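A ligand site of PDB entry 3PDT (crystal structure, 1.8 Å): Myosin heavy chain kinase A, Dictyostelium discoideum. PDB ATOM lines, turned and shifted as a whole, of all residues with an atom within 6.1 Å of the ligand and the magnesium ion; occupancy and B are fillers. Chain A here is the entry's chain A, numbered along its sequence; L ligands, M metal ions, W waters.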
ATOM      1  N   PHE A  52     -36.861  27.095   6.785  1.00  0.00           N
ATOM      2  CA  PHE A  52     -36.803  28.238   7.708  1.00  0.00           C
ATOM      3  C   PHE A  52     -36.175  29.468   7.062  1.00  0.00           C
ATOM      4  O   PHE A  52     -36.323  30.580   7.583  1.00  0.00           O
ATOM      5  CB  PHE A  52     -36.085  27.878   9.015  1.00  0.00           C
ATOM      6  CG  PHE A  52     -34.589  27.713   8.890  1.00  0.00           C
ATOM      7  CD1 PHE A  52     -33.732  28.784   9.119  1.00  0.00           C
ATOM      8  CD2 PHE A  52     -34.048  26.464   8.590  1.00  0.00           C
ATOM      9  CE1 PHE A  52     -32.345  28.625   9.017  1.00  0.00           C
ATOM     10  CE2 PHE A  52     -32.663  26.301   8.480  1.00  0.00           C
ATOM     11  CZ  PHE A  52     -31.817  27.378   8.696  1.00  0.00           C
ATOM     12  N   ALA A  53     -35.475  29.259   5.946  1.00  0.00           N
ATOM     13  CA  ALA A  53     -34.794  30.339   5.246  1.00  0.00           C
ATOM     14  C   ALA A  53     -34.593  29.955   3.780  1.00  0.00           C
ATOM     15  O   ALA A  53     -34.675  28.786   3.410  1.00  0.00           O
ATOM     16  CB  ALA A  53     -33.446  30.646   5.919  1.00  0.00           C
ATOM     17  N   GLU A  54     -34.363  30.958   2.932  1.00  0.00           N
ATOM     18  CA  GLU A  54     -34.055  30.693   1.529  1.00  0.00           C
ATOM     19  C   GLU A  54     -33.042  31.689   0.982  1.00  0.00           C
ATOM     20  O   GLU A  54     -32.911  32.809   1.489  1.00  0.00           O
ATOM     21  CB  GLU A  54     -35.328  30.646   0.679  1.00  0.00           C
ATOM     22  CG  GLU A  54     -36.144  31.932   0.641  1.00  0.00           C
ATOM     23  CD  GLU A  54     -37.084  32.030  -0.577  1.00  0.00           C
ATOM     24  OE1 GLU A  54     -37.390  30.988  -1.203  1.00  0.00           O
ATOM     25  OE2 GLU A  54     -37.518  33.159  -0.892  1.00  0.00           O
ATOM     26  N   GLY A  55     -32.315  31.262  -0.045  1.00  0.00           N
ATOM     27  CA  GLY A  55     -31.396  32.120  -0.753  1.00  0.00           C
ATOM     28  C   GLY A  55     -31.783  32.249  -2.211  1.00  0.00           C
ATOM     29  O   GLY A  55     -32.895  31.923  -2.568  1.00  0.00           O
ATOM     30  N   ALA A  56     -30.851  32.723  -3.043  1.00  0.00           N
ATOM     31  CA  ALA A  56     -31.120  32.859  -4.476  1.00  0.00           C
ATOM     32  C   ALA A  56     -31.454  31.520  -5.134  1.00  0.00           C
ATOM     33  O   ALA A  56     -32.340  31.448  -5.987  1.00  0.00           O
ATOM     34  CB  ALA A  56     -29.924  33.510  -5.173  1.00  0.00           C
ATOM     35  N   LEU A  57     -30.753  30.467  -4.727  1.00  0.00           N
ATOM     36  CA  LEU A  57     -30.832  29.177  -5.414  1.00  0.00           C
ATOM     37  C   LEU A  57     -31.482  28.060  -4.578  1.00  0.00           C
ATOM     38  O   LEU A  57     -32.046  27.108  -5.129  1.00  0.00           O
ATOM     39  CB  LEU A  57     -29.447  28.742  -5.915  1.00  0.00           C
ATOM     40  CG  LEU A  57     -28.720  29.624  -6.940  1.00  0.00           C
ATOM     41  CD1 LEU A  57     -27.285  29.159  -7.178  1.00  0.00           C
ATOM     42  CD2 LEU A  57     -29.471  29.661  -8.265  1.00  0.00           C
ATOM     43  N   ARG A  58     -31.404  28.202  -3.256  1.00  0.00           N
ATOM     44  CA  ARG A  58     -31.754  27.094  -2.361  1.00  0.00           C
ATOM     45  C   ARG A  58     -32.718  27.461  -1.235  1.00  0.00           C
ATOM     46  O   ARG A  58     -32.890  28.635  -0.909  1.00  0.00           O
ATOM     47  CB  ARG A  58     -30.459  26.514  -1.770  1.00  0.00           C
ATOM     48  CG  ARG A  58     -29.497  26.066  -2.856  1.00  0.00           C
ATOM     49  CD  ARG A  58     -28.370  25.228  -2.327  1.00  0.00           C
ATOM     50  NE  ARG A  58     -27.456  25.995  -1.487  1.00  0.00           N
ATOM     51  CZ  ARG A  58     -26.355  25.493  -0.932  1.00  0.00           C
ATOM     52  NH1 ARG A  58     -26.022  24.231  -1.141  1.00  0.00           N
ATOM     53  NH2 ARG A  58     -25.584  26.271  -0.177  1.00  0.00           N
ATOM     54  N   GLU A  59     -33.353  26.433  -0.663  1.00  0.00           N
ATOM     55  CA  GLU A  59     -34.148  26.572   0.555  1.00  0.00           C
ATOM     56  C   GLU A  59     -33.507  25.741   1.678  1.00  0.00           C
ATOM     57  O   GLU A  59     -33.011  24.643   1.417  1.00  0.00           O
ATOM     58  CB  GLU A  59     -35.592  26.133   0.300  1.00  0.00           C
ATOM     59  CG  GLU A  59     -36.340  27.073  -0.644  1.00  0.00           C
ATOM     60  CD  GLU A  59     -37.803  26.698  -0.846  1.00  0.00           C
ATOM     61  OE1 GLU A  59     -38.093  25.573  -1.299  1.00  0.00           O
ATOM     62  OE2 GLU A  59     -38.681  27.550  -0.555  1.00  0.00           O
ATOM     63  N   ALA A  60     -33.535  26.266   2.897  1.00  0.00           N
ATOM     64  CA  ALA A  60     -32.830  25.664   4.041  1.00  0.00           C
ATOM     65  C   ALA A  60     -33.837  25.113   5.053  1.00  0.00           C
ATOM     66  O   ALA A  60     -34.822  25.783   5.378  1.00  0.00           O
ATOM     67  CB  ALA A  60     -31.908  26.682   4.688  1.00  0.00           C
ATOM     68  N   VAL A 109     -28.527  21.549   9.239  1.00  0.00           N
ATOM     69  CA  VAL A 109     -29.250  22.211   8.162  1.00  0.00           C
ATOM     70  C   VAL A 109     -29.202  21.392   6.887  1.00  0.00           C
ATOM     71  O   VAL A 109     -28.130  20.918   6.503  1.00  0.00           O
ATOM     72  CB  VAL A 109     -28.680  23.634   7.915  1.00  0.00           C
ATOM     73  CG1 VAL A 109     -29.324  24.290   6.673  1.00  0.00           C
ATOM     74  CG2 VAL A 109     -28.904  24.487   9.137  1.00  0.00           C
ATOM     75  N   LYS A 111     -30.216  21.472   2.727  1.00  0.00           N
ATOM     76  CA  LYS A 111     -30.471  22.430   1.654  1.00  0.00           C
ATOM     77  C   LYS A 111     -30.841  21.743   0.360  1.00  0.00           C
ATOM     78  O   LYS A 111     -30.145  20.823  -0.092  1.00  0.00           O
ATOM     79  CB  LYS A 111     -29.262  23.357   1.446  1.00  0.00           C
ATOM     80  CG  LYS A 111     -29.024  24.318   2.618  1.00  0.00           C
ATOM     81  CD  LYS A 111     -27.765  25.138   2.415  1.00  0.00           C
ATOM     82  CE  LYS A 111     -27.467  26.013   3.636  1.00  0.00           C
ATOM     83  NZ  LYS A 111     -26.206  26.796   3.428  1.00  0.00           N
ATOM     84  N   ASP A 129     -20.497  21.305  -5.584  1.00  0.00           N
ATOM     85  CA  ASP A 129     -20.804  22.318  -4.556  1.00  0.00           C
ATOM     86  C   ASP A 129     -20.104  22.004  -3.232  1.00  0.00           C
ATOM     87  O   ASP A 129     -19.513  22.883  -2.596  1.00  0.00           O
ATOM     88  CB  ASP A 129     -22.325  22.390  -4.311  1.00  0.00           C
ATOM     89  CG  ASP A 129     -23.080  22.979  -5.494  1.00  0.00           C
ATOM     90  OD1 ASP A 129     -22.449  23.674  -6.314  1.00  0.00           O
ATOM     91  OD2 ASP A 129     -24.312  22.748  -5.594  1.00  0.00           O
ATOM     92  N   MET A 132     -16.304  22.377  -3.473  1.00  0.00           N
ATOM     93  CA  MET A 132     -16.004  23.801  -3.427  1.00  0.00           C
ATOM     94  C   MET A 132     -15.944  24.310  -1.994  1.00  0.00           C
ATOM     95  O   MET A 132     -15.015  25.020  -1.631  1.00  0.00           O
ATOM     96  CB  MET A 132     -17.016  24.627  -4.230  1.00  0.00           C
ATOM     97  CG  MET A 132     -16.823  26.148  -4.069  1.00  0.00           C
ATOM     98  SD  MET A 132     -17.704  27.076  -5.293  1.00  0.00           S
ATOM     99  CE  MET A 132     -19.403  26.908  -4.753  1.00  0.00           C
ATOM    100  N   LEU A 155     -17.636  26.079   7.513  1.00  0.00           N
ATOM    101  CA  LEU A 155     -18.327  24.854   7.910  1.00  0.00           C
ATOM    102  C   LEU A 155     -18.019  23.713   6.943  1.00  0.00           C
ATOM    103  O   LEU A 155     -17.803  23.934   5.748  1.00  0.00           O
ATOM    104  CB  LEU A 155     -19.839  25.084   7.894  1.00  0.00           C
ATOM    105  CG  LEU A 155     -20.453  26.000   8.953  1.00  0.00           C
ATOM    106  CD1 LEU A 155     -21.934  26.027   8.732  1.00  0.00           C
ATOM    107  CD2 LEU A 155     -20.136  25.492  10.362  1.00  0.00           C
ATOM    108  N   GLU A 179     -25.229  20.586   6.265  1.00  0.00           N
ATOM    109  CA  GLU A 179     -24.189  21.390   6.907  1.00  0.00           C
ATOM    110  C   GLU A 179     -24.594  21.612   8.354  1.00  0.00           C
ATOM    111  O   GLU A 179     -25.775  21.478   8.695  1.00  0.00           O
ATOM    112  CB  GLU A 179     -24.091  22.758   6.244  1.00  0.00           C
ATOM    113  CG  GLU A 179     -23.181  22.809   5.031  1.00  0.00           C
ATOM    114  CD  GLU A 179     -23.584  23.888   4.038  1.00  0.00           C
ATOM    115  OE1 GLU A 179     -24.686  24.475   4.170  1.00  0.00           O
ATOM    116  OE2 GLU A 179     -22.800  24.141   3.088  1.00  0.00           O
ATOM    117  N   PRO A 180     -23.624  21.955   9.226  1.00  0.00           N
ATOM    118  CA  PRO A 180     -24.002  22.244  10.611  1.00  0.00           C
ATOM    119  C   PRO A 180     -24.896  23.499  10.733  1.00  0.00           C
ATOM    120  O   PRO A 180     -24.918  24.336   9.821  1.00  0.00           O
ATOM    121  CB  PRO A 180     -22.652  22.496  11.310  1.00  0.00           C
ATOM    122  CG  PRO A 180     -21.663  21.734  10.482  1.00  0.00           C
ATOM    123  CD  PRO A 180     -22.151  21.937   9.070  1.00  0.00           C
ATOM    124  N   LEU A 181     -25.633  23.601  11.830  1.00  0.00           N
ATOM    125  CA  LEU A 181     -26.459  24.789  12.104  1.00  0.00           C
ATOM    126  C   LEU A 181     -25.630  25.918  12.721  1.00  0.00           C
ATOM    127  O   LEU A 181     -24.947  25.716  13.732  1.00  0.00           O
ATOM    128  CB  LEU A 181     -27.655  24.429  13.013  1.00  0.00           C
ATOM    129  CG  LEU A 181     -28.551  25.576  13.517  1.00  0.00           C
ATOM    130  CD1 LEU A 181     -29.413  26.117  12.384  1.00  0.00           C
ATOM    131  CD2 LEU A 181     -29.416  25.140  14.701  1.00  0.00           C
ATOM    132  N   LEU A 182     -25.710  27.102  12.110  1.00  0.00           N
ATOM    133  CA  LEU A 182     -25.072  28.299  12.649  1.00  0.00           C
ATOM    134  C   LEU A 182     -26.002  28.927  13.675  1.00  0.00           C
ATOM    135  O   LEU A 182     -27.181  29.134  13.406  1.00  0.00           O
ATOM    136  CB  LEU A 182     -24.761  29.307  11.551  1.00  0.00           C
ATOM    137  CG  LEU A 182     -23.635  28.939  10.557  1.00  0.00           C
ATOM    138  CD1 LEU A 182     -23.550  29.940   9.403  1.00  0.00           C
ATOM    139  CD2 LEU A 182     -22.285  28.829  11.237  1.00  0.00           C
ATOM    140  N   VAL A 183     -25.462  29.203  14.842  1.00  0.00           N
ATOM    141  CA  VAL A 183     -26.226  29.787  15.940  1.00  0.00           C
ATOM    142  C   VAL A 183     -25.739  31.240  16.096  1.00  0.00           C
ATOM    143  O   VAL A 183     -24.543  31.463  16.323  1.00  0.00           O
ATOM    144  CB  VAL A 183     -25.986  28.996  17.242  1.00  0.00           C
ATOM    145  CG1 VAL A 183     -26.766  29.607  18.410  1.00  0.00           C
ATOM    146  CG2 VAL A 183     -26.351  27.520  17.033  1.00  0.00           C
ATOM    147  N   PHE A 186     -26.880  35.687  11.355  1.00  0.00           N
ATOM    148  CA  PHE A 186     -26.316  35.354  10.048  1.00  0.00           C
ATOM    149  C   PHE A 186     -26.202  36.639   9.250  1.00  0.00           C
ATOM    150  O   PHE A 186     -27.191  37.389   9.117  1.00  0.00           O
ATOM    151  CB  PHE A 186     -27.240  34.377   9.324  1.00  0.00           C
ATOM    152  CG  PHE A 186     -26.628  33.733   8.111  1.00  0.00           C
ATOM    153  CD1 PHE A 186     -26.156  32.426   8.162  1.00  0.00           C
ATOM    154  CD2 PHE A 186     -26.534  34.434   6.907  1.00  0.00           C
ATOM    155  CE1 PHE A 186     -25.607  31.816   7.039  1.00  0.00           C
ATOM    156  CE2 PHE A 186     -25.974  33.831   5.778  1.00  0.00           C
ATOM    157  CZ  PHE A 186     -25.521  32.515   5.850  1.00  0.00           C
ATOM    158  N   LYS A 188     -24.353  38.394   5.574  1.00  0.00           N
ATOM    159  CA  LYS A 188     -23.600  38.360   4.327  1.00  0.00           C
ATOM    160  C   LYS A 188     -22.634  39.540   4.271  1.00  0.00           C
ATOM    161  O   LYS A 188     -23.050  40.682   4.445  1.00  0.00           O
ATOM    162  CB  LYS A 188     -24.549  38.443   3.142  1.00  0.00           C
ATOM    163  CG  LYS A 188     -23.968  37.951   1.839  1.00  0.00           C
ATOM    164  CD  LYS A 188     -25.064  37.784   0.811  1.00  0.00           C
ATOM    165  CE  LYS A 188     -24.538  37.154  -0.445  1.00  0.00           C
ATOM    166  NZ  LYS A 188     -25.616  37.016  -1.458  1.00  0.00           N
ATOM    167  N   ASP A 222     -18.771  35.680  -1.681  1.00  0.00           N
ATOM    168  CA  ASP A 222     -19.963  35.248  -0.931  1.00  0.00           C
ATOM    169  C   ASP A 222     -19.568  34.842   0.500  1.00  0.00           C
ATOM    170  O   ASP A 222     -19.976  33.804   1.010  1.00  0.00           O
ATOM    171  CB  ASP A 222     -20.698  34.083  -1.633  1.00  0.00           C
ATOM    172  CG  ASP A 222     -21.921  34.524  -2.448  1.00  0.00           C
ATOM    173  OD1 ASP A 222     -22.467  35.637  -2.194  1.00  0.00           O
ATOM    174  OD2 ASP A 222     -22.336  33.758  -3.341  1.00  0.00           O
ATOM    175  N   GLN A 224     -20.032  34.742   4.084  1.00  0.00           N
ATOM    176  CA  GLN A 224     -21.273  34.897   4.812  1.00  0.00           C
ATOM    177  C   GLN A 224     -21.322  33.919   5.956  1.00  0.00           C
ATOM    178  O   GLN A 224     -20.879  32.781   5.820  1.00  0.00           O
ATOM    179  CB  GLN A 224     -22.413  34.581   3.854  1.00  0.00           C
ATOM    180  CG  GLN A 224     -23.758  35.111   4.266  1.00  0.00           C
ATOM    181  CD  GLN A 224     -24.848  34.788   3.243  1.00  0.00           C
ATOM    182  OE1 GLN A 224     -24.708  33.847   2.459  1.00  0.00           O
ATOM    183  NE2 GLN A 224     -25.935  35.561   3.259  1.00  0.00           N
ATOM    184  N   THR A 231     -20.276  30.023   5.700  1.00  0.00           N
ATOM    185  CA  THR A 231     -20.825  28.930   4.884  1.00  0.00           C
ATOM    186  C   THR A 231     -21.285  29.429   3.503  1.00  0.00           C
ATOM    187  O   THR A 231     -21.341  30.646   3.246  1.00  0.00           O
ATOM    188  CB  THR A 231     -21.946  28.154   5.647  1.00  0.00           C
ATOM    189  OG1 THR A 231     -22.150  26.869   5.021  1.00  0.00           O
ATOM    190  CG2 THR A 231     -23.278  28.949   5.654  1.00  0.00           C
ATOM    191  N   ASP A 232     -21.596  28.467   2.635  1.00  0.00           N
ATOM    192  CA  ASP A 232     -21.955  28.728   1.242  1.00  0.00           C
ATOM    193  C   ASP A 232     -21.152  29.841   0.553  1.00  0.00           C
ATOM    194  O   ASP A 232     -21.739  30.766  -0.024  1.00  0.00           O
ATOM    195  CB  ASP A 232     -23.470  28.933   1.090  1.00  0.00           C
ATOM    196  CG  ASP A 232     -23.920  28.816  -0.358  1.00  0.00           C
ATOM    197  OD1 ASP A 232     -23.165  28.265  -1.197  1.00  0.00           O
ATOM    198  OD2 ASP A 232     -25.049  29.277  -0.671  1.00  0.00           O
ATOM    199  N   PRO A 233     -19.808  29.740   0.571  1.00  0.00           N
ATOM    200  CA  PRO A 233     -19.015  30.680  -0.213  1.00  0.00           C
ATOM    201  C   PRO A 233     -19.091  30.356  -1.687  1.00  0.00           C
ATOM    202  O   PRO A 233     -19.681  29.325  -2.068  1.00  0.00           O
ATOM    203  CB  PRO A 233     -17.590  30.417   0.284  1.00  0.00           C
ATOM    204  CG  PRO A 233     -17.603  28.947   0.601  1.00  0.00           C
ATOM    205  CD  PRO A 233     -18.961  28.700   1.198  1.00  0.00           C
ATOM    206  N   GLN A 234     -18.500  31.202  -2.513  1.00  0.00           N
ATOM    207  CA  GLN A 234     -18.469  30.970  -3.955  1.00  0.00           C
ATOM    208  C   GLN A 234     -17.103  31.326  -4.517  1.00  0.00           C
ATOM    209  O   GLN A 234     -16.538  32.357  -4.164  1.00  0.00           O
ATOM    210  CB  GLN A 234     -19.555  31.810  -4.644  1.00  0.00           C
ATOM    211  CG  GLN A 234     -19.617  31.628  -6.167  1.00  0.00           C
ATOM    212  CD  GLN A 234     -19.915  30.208  -6.579  1.00  0.00           C
ATOM    213  OE1 GLN A 234     -20.901  29.625  -6.125  1.00  0.00           O
ATOM    214  NE2 GLN A 234     -19.079  29.630  -7.469  1.00  0.00           N
ATOM    215  N   ILE A 235     -16.590  30.444  -5.386  1.00  0.00           N
ATOM    216  CA  ILE A 235     -15.334  30.679  -6.101  1.00  0.00           C
ATOM    217  C   ILE A 235     -15.599  31.116  -7.545  1.00  0.00           C
ATOM    218  O   ILE A 235     -16.479  30.551  -8.229  1.00  0.00           O
ATOM    219  CB  ILE A 235     -14.445  29.395  -6.060  1.00  0.00           C
ATOM    220  CG1 ILE A 235     -13.964  29.140  -4.621  1.00  0.00           C
ATOM    221  CG2 ILE A 235     -13.255  29.499  -7.048  1.00  0.00           C
ATOM    222  CD1 ILE A 235     -13.190  27.815  -4.452  1.00  0.00           C
HETATM  223  P1  LIG L   1     -27.376  32.478   0.416  1.00  0.00           P
HETATM  224  O1  LIG L   1     -28.486  32.210  -0.549  1.00  0.00           O
HETATM  225  O2  LIG L   1     -27.713  33.440   1.534  1.00  0.00           O
HETATM  226  O3  LIG L   1     -26.065  32.794  -0.260  1.00  0.00           O
HETATM  227  P2  LIG L   1     -27.917  29.702   1.175  1.00  0.00           P
HETATM  228  O4  LIG L   1     -28.806  29.597  -0.025  1.00  0.00           O
HETATM  229  O5  LIG L   1     -26.883  28.633   1.475  1.00  0.00           O
HETATM  230  O6  LIG L   1     -27.077  31.074   1.170  1.00  0.00           O
HETATM  231  O7  LIG L   1     -28.834  29.787   2.494  1.00  0.00           O
HETATM  232  C1  LIG L   1     -30.048  30.532   2.463  1.00  0.00           C
HETATM  233  C2  LIG L   1     -30.270  31.162   3.827  1.00  0.00           C
HETATM  234  O8  LIG L   1     -30.279  30.156   4.862  1.00  0.00           O
HETATM  235  C3  LIG L   1     -29.161  32.107   4.214  1.00  0.00           C
HETATM  236  O9  LIG L   1     -29.347  33.417   3.683  1.00  0.00           O
HETATM  237  C4  LIG L   1     -29.206  32.101   5.718  1.00  0.00           C
HETATM  238  O10 LIG L   1     -30.269  32.950   6.169  1.00  0.00           O
HETATM  239  C5  LIG L   1     -29.623  30.682   6.018  1.00  0.00           C
HETATM  240  N1  LIG L   1     -28.507  29.741   6.258  1.00  0.00           N
HETATM  241  C6  LIG L   1     -27.699  29.214   5.305  1.00  0.00           C
HETATM  242  N2  LIG L   1     -26.823  28.354   5.849  1.00  0.00           N
HETATM  243  C7  LIG L   1     -27.101  28.290   7.176  1.00  0.00           C
HETATM  244  C8  LIG L   1     -26.556  27.563   8.339  1.00  0.00           C
HETATM  245  N3  LIG L   1     -25.519  26.697   8.176  1.00  0.00           N
HETATM  246  N4  LIG L   1     -27.115  27.783   9.563  1.00  0.00           N
HETATM  247  C9  LIG L   1     -28.155  28.636   9.721  1.00  0.00           C
HETATM  248  N5  LIG L   1     -28.716  29.342   8.709  1.00  0.00           N
HETATM  249  C10 LIG L   1     -28.227  29.200   7.442  1.00  0.00           C
HETATM  250 MG    MG M   1     -22.025  28.711  -3.487  1.00  0.00          MG
HETATM  251  O   HOH W   1     -22.628  26.063  -4.378  1.00  0.00           O
HETATM  252  O   HOH W   2     -31.852  34.562   4.068  1.00  0.00           O
HETATM  253  O   HOH W   3     -22.646  31.143  -2.511  1.00  0.00           O
HETATM  254  O   HOH W   4     -29.657  35.006  -0.105  1.00  0.00           O
HETATM  255  O   HOH W   5     -29.805  31.424  10.297  1.00  0.00           O
HETATM  256  O   HOH W   6     -25.579  31.332  -3.038  1.00  0.00           O
HETATM  257  O   HOH W   7     -30.899  33.377   8.731  1.00  0.00           O
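CZ of Phe 52 touches N5 of the ligand (3.7 Å). Ala 53 touches the ligand. Glu 54 touches the ligand. CA of Gly 55 touches O1 of the ligand (2.9 Å). Ala 60 touches the ligand. CG2 of Val 109 touches N4 of the ligand, 3.8 Å away. Leu 155 touches the ligand (CD1 to N3, 3.7 Å). Leu 181 touches the ligand. CE1 of Phe 186 touches N1 of the ligand (3.7 Å). Thr 231 touches the ligand (CG2 to N2, 3.6 Å). Hydrophobic or aromatic side chains that line the ligand: Phe 52, Ala 53, Ala 60, Val 109, Leu 155, Leu 181, Leu 182 and Phe 186. Of the 28 residues printed, 17 come within 4 Å of the ligand. The nearest printed residue that does not touch the ligand is Lys 188 (4.4 Å).
Met 132 touches the magnesium ion. Gln 234 touches the magnesium ion.
O5 of the ligand sits close to OD2 of Asp 232 (2.9 Å). The side-chain amino group (NZ) of Lys 111 is in salt-bridge range of an oxygen (O5) of the ligand, at 2.8 Å. N3 of the ligand sits at hydrogen-bond distance from O of Pro 180. The backbone NH (N) of Leu 182 lies within hydrogen-bond range of a nitrogen (N4) of the ligand (3.0 Å). NH2 of Arg 58 is in salt-bridge range of O5 of the ligand (3.2 Å). O2 of the ligand lies close to OE1 of Gln 224, 3.2 Å away. O1 of the ligand sits at hydrogen-bond distance from N of Ala 56 (3.5 Å).
The magnesium ion is bound by OD1 of Asp 232 (2.6 Å). The magnesium ion has one donor atom within binding distance. Slightly farther from the magnesium ion lies water W3 (2.7 Å). Slightly farther from the magnesium ion lies the backbone carbonyl oxygen (O) of Pro 233 (2.8 Å).
The side-chain carboxylate (OD2) of Asp 232 lies within salt-bridge range of the guanidinium group (NH2) of Arg 58 (3.1 Å). The side-chain amino group (NZ) of Lys 111 is in salt-bridge range of the side-chain carboxylate (OE1) of Glu 179, 2.9 Å away. The side-chain amide nitrogen (NE2) of Gln 234 lies within hydrogen-bond range of the side-chain sulfur (SD) of Met 132 (3.6 Å). The backbone carbonyl oxygen of Gln 224 sits at hydrogen-bond distance from the backbone NH of Thr 231 (2.8 Å). SD of Met 132 sits at hydrogen-bond distance from N of Ile 235. The side-chain hydroxyl (OG1) of Thr 231 sits at hydrogen-bond distance from the side-chain carboxylate (OE2) of Glu 179. N of Phe 52 is in hydrogen-bond range of O of Ala 60. O of Glu 179 lies within hydrogen-bond range of N of Val 109, 2.8 Å away.
Water W3 bridges O of Asp 232 (2.7 Å) and OD2 of Asp 222 (2.8 Å). Water W2 lies within hydrogen-bond range of O9 of the ligand and O of Glu 54. Water W6 bridges O3 of the ligand (3.2 Å) and OD2 of Asp 232 (3.2 Å).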
